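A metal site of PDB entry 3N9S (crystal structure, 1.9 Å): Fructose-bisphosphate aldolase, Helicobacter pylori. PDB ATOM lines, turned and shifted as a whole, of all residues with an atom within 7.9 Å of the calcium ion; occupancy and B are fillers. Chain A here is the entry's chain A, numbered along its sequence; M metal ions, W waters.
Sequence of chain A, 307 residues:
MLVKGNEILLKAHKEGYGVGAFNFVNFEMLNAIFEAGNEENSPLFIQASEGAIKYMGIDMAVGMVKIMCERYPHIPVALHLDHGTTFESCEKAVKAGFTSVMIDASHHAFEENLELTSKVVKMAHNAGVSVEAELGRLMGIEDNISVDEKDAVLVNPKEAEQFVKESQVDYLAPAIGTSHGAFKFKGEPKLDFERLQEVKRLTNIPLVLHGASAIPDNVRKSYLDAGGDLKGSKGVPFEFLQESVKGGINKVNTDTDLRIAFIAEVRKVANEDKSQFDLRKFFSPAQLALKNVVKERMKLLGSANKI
Within 4 Å of the calcium ion: Asp 104, Ser 106 and Glu 134.
The side-chain carboxylate (OD2) of Asp 104 lies close to a ring nitrogen (ND1) of His 83, 2.7 Å away.
The backbone NH (N) of Asp 104 is in hydrogen-bond range of the backbone carbonyl oxygen (O) of Gly 84 (2.8 Å).
The side-chain hydroxyl (OG) of Ser 106 lies close to the backbone carbonyl oxygen (O) of Gly 136 (3.5 Å).
The calcium ion is bound by the side-chain carboxylate (OD2) of Asp 104 (2.5 Å), water W1 (2.6 Å), the side-chain hydroxyl (OG) of Ser 106 (2.6 Å), the side-chain carboxylate (OE1) of Glu 134 (2.6 Å), the side-chain carboxylate (OD1) of Asp 104 (2.6 Å), water W3 (2.7 Å) and water W2 (2.7 Å).
The calcium ion has seven donor atoms within binding distance.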
ATOM      1  N   HIS A  83      18.001  -9.723 -30.185  1.00  0.00           N
ATOM      2  CA  HIS A  83      16.760 -10.318 -29.696  1.00  0.00           C
ATOM      3  C   HIS A  83      15.935 -11.044 -30.766  1.00  0.00           C
ATOM      4  O   HIS A  83      14.760 -10.755 -30.954  1.00  0.00           O
ATOM      5  CB  HIS A  83      15.905  -9.252 -29.009  1.00  0.00           C
ATOM      6  CG  HIS A  83      16.511  -8.758 -27.732  1.00  0.00           C
ATOM      7  ND1 HIS A  83      16.536  -9.520 -26.583  1.00  0.00           N
ATOM      8  CD2 HIS A  83      17.149  -7.608 -27.426  1.00  0.00           C
ATOM      9  CE1 HIS A  83      17.147  -8.855 -25.632  1.00  0.00           C
ATOM     10  NE2 HIS A  83      17.524  -7.692 -26.109  1.00  0.00           N
ATOM     11  N   GLY A  84      16.555 -11.999 -31.449  1.00  0.00           N
ATOM     12  CA  GLY A  84      15.801 -12.949 -32.253  1.00  0.00           C
ATOM     13  C   GLY A  84      14.844 -13.736 -31.372  1.00  0.00           C
ATOM     14  O   GLY A  84      15.221 -14.185 -30.289  1.00  0.00           O
ATOM     15  N   MET A 102      21.379 -13.387 -32.090  1.00  0.00           N
ATOM     16  CA  MET A 102      20.910 -13.696 -30.753  1.00  0.00           C
ATOM     17  C   MET A 102      19.592 -14.443 -30.821  1.00  0.00           C
ATOM     18  O   MET A 102      18.627 -13.941 -31.393  1.00  0.00           O
ATOM     19  CB  MET A 102      20.675 -12.432 -29.951  1.00  0.00           C
ATOM     20  CG  MET A 102      20.362 -12.732 -28.503  1.00  0.00           C
ATOM     21  SD  MET A 102      19.597 -11.359 -27.627  1.00  0.00           S
ATOM     22  CE  MET A 102      19.647 -11.968 -25.935  1.00  0.00           C
ATOM     23  N   ILE A 103      19.546 -15.629 -30.228  1.00  0.00           N
ATOM     24  CA  ILE A 103      18.263 -16.286 -30.016  1.00  0.00           C
ATOM     25  C   ILE A 103      17.884 -16.066 -28.556  1.00  0.00           C
ATOM     26  O   ILE A 103      18.521 -16.593 -27.648  1.00  0.00           O
ATOM     27  CB  ILE A 103      18.309 -17.777 -30.374  1.00  0.00           C
ATOM     28  CG1 ILE A 103      16.989 -18.457 -29.977  1.00  0.00           C
ATOM     29  CG2 ILE A 103      19.484 -18.460 -29.696  1.00  0.00           C
ATOM     30  CD1 ILE A 103      15.783 -17.955 -30.770  1.00  0.00           C
ATOM     31  N   ASP A 104      16.858 -15.262 -28.345  1.00  0.00           N
ATOM     32  CA  ASP A 104      16.457 -14.895 -27.003  1.00  0.00           C
ATOM     33  C   ASP A 104      15.206 -15.657 -26.560  1.00  0.00           C
ATOM     34  O   ASP A 104      14.093 -15.328 -26.955  1.00  0.00           O
ATOM     35  CB  ASP A 104      16.211 -13.391 -26.932  1.00  0.00           C
ATOM     36  CG  ASP A 104      15.758 -12.945 -25.574  1.00  0.00           C
ATOM     37  OD1 ASP A 104      15.736 -13.778 -24.638  1.00  0.00           O
ATOM     38  OD2 ASP A 104      15.434 -11.745 -25.424  1.00  0.00           O
ATOM     39  N   ALA A 105      15.411 -16.667 -25.721  1.00  0.00           N
ATOM     40  CA  ALA A 105      14.338 -17.497 -25.211  1.00  0.00           C
ATOM     41  C   ALA A 105      14.422 -17.516 -23.689  1.00  0.00           C
ATOM     42  O   ALA A 105      14.092 -18.507 -23.046  1.00  0.00           O
ATOM     43  CB  ALA A 105      14.455 -18.887 -25.770  1.00  0.00           C
ATOM     44  N   SER A 106      14.876 -16.418 -23.119  1.00  0.00           N
ATOM     45  CA  SER A 106      15.127 -16.358 -21.684  1.00  0.00           C
ATOM     46  C   SER A 106      13.820 -16.420 -20.902  1.00  0.00           C
ATOM     47  O   SER A 106      13.804 -16.796 -19.736  1.00  0.00           O
ATOM     48  CB  SER A 106      15.869 -15.063 -21.356  1.00  0.00           C
ATOM     49  OG  SER A 106      14.992 -13.962 -21.448  1.00  0.00           O
ATOM     50  N   HIS A 107      12.718 -16.038 -21.543  1.00  0.00           N
ATOM     51  CA  HIS A 107      11.410 -16.091 -20.905  1.00  0.00           C
ATOM     52  C   HIS A 107      10.854 -17.517 -20.911  1.00  0.00           C
ATOM     53  O   HIS A 107       9.877 -17.807 -20.235  1.00  0.00           O
ATOM     54  CB  HIS A 107      10.422 -15.135 -21.576  1.00  0.00           C
ATOM     55  CG  HIS A 107      10.327 -15.316 -23.058  1.00  0.00           C
ATOM     56  ND1 HIS A 107      11.287 -14.840 -23.924  1.00  0.00           N
ATOM     57  CD2 HIS A 107       9.382 -15.902 -23.836  1.00  0.00           C
ATOM     58  CE1 HIS A 107      10.939 -15.133 -25.169  1.00  0.00           C
ATOM     59  NE2 HIS A 107       9.791 -15.784 -25.137  1.00  0.00           N
ATOM     60  N   HIS A 108      11.478 -18.401 -21.692  1.00  0.00           N
ATOM     61  CA  HIS A 108      11.081 -19.805 -21.685  1.00  0.00           C
ATOM     62  C   HIS A 108      11.735 -20.540 -20.526  1.00  0.00           C
ATOM     63  O   HIS A 108      12.752 -20.100 -19.986  1.00  0.00           O
ATOM     64  CB  HIS A 108      11.491 -20.500 -22.979  1.00  0.00           C
ATOM     65  CG  HIS A 108      10.680 -20.094 -24.170  1.00  0.00           C
ATOM     66  ND1 HIS A 108      11.168 -19.278 -25.168  1.00  0.00           N
ATOM     67  CD2 HIS A 108       9.399 -20.386 -24.515  1.00  0.00           C
ATOM     68  CE1 HIS A 108      10.228 -19.080 -26.078  1.00  0.00           C
ATOM     69  NE2 HIS A 108       9.144 -19.743 -25.707  1.00  0.00           N
ATOM     70  N   GLU A 134      20.536 -16.089 -23.940  1.00  0.00           N
ATOM     71  CA  GLU A 134      20.327 -15.299 -22.732  1.00  0.00           C
ATOM     72  C   GLU A 134      19.679 -16.114 -21.612  1.00  0.00           C
ATOM     73  O   GLU A 134      18.791 -16.933 -21.869  1.00  0.00           O
ATOM     74  CB  GLU A 134      19.433 -14.090 -23.046  1.00  0.00           C
ATOM     75  CG  GLU A 134      19.222 -13.157 -21.859  1.00  0.00           C
ATOM     76  CD  GLU A 134      18.510 -11.875 -22.242  1.00  0.00           C
ATOM     77  OE1 GLU A 134      17.673 -11.905 -23.162  1.00  0.00           O
ATOM     78  OE2 GLU A 134      18.793 -10.829 -21.623  1.00  0.00           O
ATOM     79  N   LEU A 135      20.134 -15.884 -20.395  1.00  0.00           N
ATOM     80  CA  LEU A 135      19.553 -16.482 -19.204  1.00  0.00           C
ATOM     81  C   LEU A 135      19.266 -15.397 -18.185  1.00  0.00           C
ATOM     82  O   LEU A 135      20.091 -14.493 -17.986  1.00  0.00           O
ATOM     83  CB  LEU A 135      20.507 -17.500 -18.590  1.00  0.00           C
ATOM     84  CG  LEU A 135      20.678 -18.780 -19.402  1.00  0.00           C
ATOM     85  CD1 LEU A 135      21.896 -19.534 -18.908  1.00  0.00           C
ATOM     86  CD2 LEU A 135      19.408 -19.640 -19.328  1.00  0.00           C
ATOM     87  N   GLY A 136      18.120 -15.480 -17.540  1.00  0.00           N
ATOM     88  CA  GLY A 136      17.713 -14.482 -16.570  1.00  0.00           C
ATOM     89  C   GLY A 136      16.742 -13.498 -17.187  1.00  0.00           C
ATOM     90  O   GLY A 136      16.578 -13.446 -18.406  1.00  0.00           O
ATOM     91  N   ARG A 137      16.100 -12.709 -16.333  1.00  0.00           N
ATOM     92  CA  ARG A 137      15.137 -11.712 -16.768  1.00  0.00           C
ATOM     93  C   ARG A 137      15.783 -10.329 -16.683  1.00  0.00           C
ATOM     94  O   ARG A 137      16.457 -10.004 -15.705  1.00  0.00           O
ATOM     95  CB  ARG A 137      13.890 -11.769 -15.878  1.00  0.00           C
ATOM     96  CG  ARG A 137      12.684 -11.061 -16.465  1.00  0.00           C
ATOM     97  CD  ARG A 137      11.434 -11.368 -15.657  1.00  0.00           C
ATOM     98  NE  ARG A 137      10.245 -10.672 -16.159  1.00  0.00           N
ATOM     99  CZ  ARG A 137       9.594  -9.715 -15.503  1.00  0.00           C
ATOM    100  NH1 ARG A 137       8.539  -9.146 -16.052  1.00  0.00           N
ATOM    101  NH2 ARG A 137      10.000  -9.328 -14.298  1.00  0.00           N
ATOM    102  N   LEU A 138      15.590  -9.537 -17.724  1.00  0.00           N
ATOM    103  CA  LEU A 138      16.216  -8.213 -17.824  1.00  0.00           C
ATOM    104  C   LEU A 138      15.391  -7.148 -17.126  1.00  0.00           C
ATOM    105  O   LEU A 138      14.917  -6.213 -17.769  1.00  0.00           O
ATOM    106  CB  LEU A 138      16.370  -7.817 -19.284  1.00  0.00           C
ATOM    107  CG  LEU A 138      17.670  -8.189 -19.963  1.00  0.00           C
ATOM    108  CD1 LEU A 138      17.602  -7.744 -21.420  1.00  0.00           C
ATOM    109  CD2 LEU A 138      18.856  -7.559 -19.243  1.00  0.00           C
ATOM    110  N   ALA A 173      24.408 -13.858 -22.529  1.00  0.00           N
ATOM    111  CA  ALA A 173      23.939 -12.644 -21.872  1.00  0.00           C
ATOM    112  C   ALA A 173      23.318 -13.031 -20.542  1.00  0.00           C
ATOM    113  O   ALA A 173      22.187 -13.501 -20.499  1.00  0.00           O
ATOM    114  CB  ALA A 173      22.905 -11.929 -22.745  1.00  0.00           C
ATOM    115  N   HIS A 180      16.316  -2.845 -20.297  1.00  0.00           N
ATOM    116  CA  HIS A 180      16.282  -1.946 -21.438  1.00  0.00           C
ATOM    117  C   HIS A 180      15.681  -0.594 -21.093  1.00  0.00           C
ATOM    118  O   HIS A 180      14.773  -0.506 -20.256  1.00  0.00           O
ATOM    119  CB  HIS A 180      15.475  -2.558 -22.567  1.00  0.00           C
ATOM    120  CG  HIS A 180      16.124  -3.764 -23.166  1.00  0.00           C
ATOM    121  ND1 HIS A 180      15.402  -4.811 -23.685  1.00  0.00           N
ATOM    122  CD2 HIS A 180      17.422  -4.084 -23.323  1.00  0.00           C
ATOM    123  CE1 HIS A 180      16.230  -5.724 -24.147  1.00  0.00           C
ATOM    124  NE2 HIS A 180      17.466  -5.312 -23.933  1.00  0.00           N
ATOM    125  N   HIS A 210      23.167  -6.594 -21.634  1.00  0.00           N
ATOM    126  CA  HIS A 210      22.068  -5.830 -22.249  1.00  0.00           C
ATOM    127  C   HIS A 210      21.689  -4.710 -21.321  1.00  0.00           C
ATOM    128  O   HIS A 210      22.027  -4.760 -20.139  1.00  0.00           O
ATOM    129  CB  HIS A 210      20.853  -6.738 -22.471  1.00  0.00           C
ATOM    130  CG  HIS A 210      21.039  -7.699 -23.596  1.00  0.00           C
ATOM    131  ND1 HIS A 210      20.242  -7.687 -24.727  1.00  0.00           N
ATOM    132  CD2 HIS A 210      21.940  -8.688 -23.784  1.00  0.00           C
ATOM    133  CE1 HIS A 210      20.642  -8.635 -25.558  1.00  0.00           C
ATOM    134  NE2 HIS A 210      21.670  -9.257 -25.007  1.00  0.00           N
HETATM  135 CA    CA M   1      15.072 -11.846 -22.951  1.00  0.00          CA
HETATM  136 ZN    ZN M   2      18.820  -6.237 -25.221  1.00  0.00          ZN
HETATM  137  O   HOH W   1      12.628 -12.373 -23.524  1.00  0.00           O
HETATM  138  O   HOH W   2      15.451 -11.126 -20.347  1.00  0.00           O
HETATM  139  O   HOH W   3      14.721  -9.221 -23.200  1.00  0.00           O
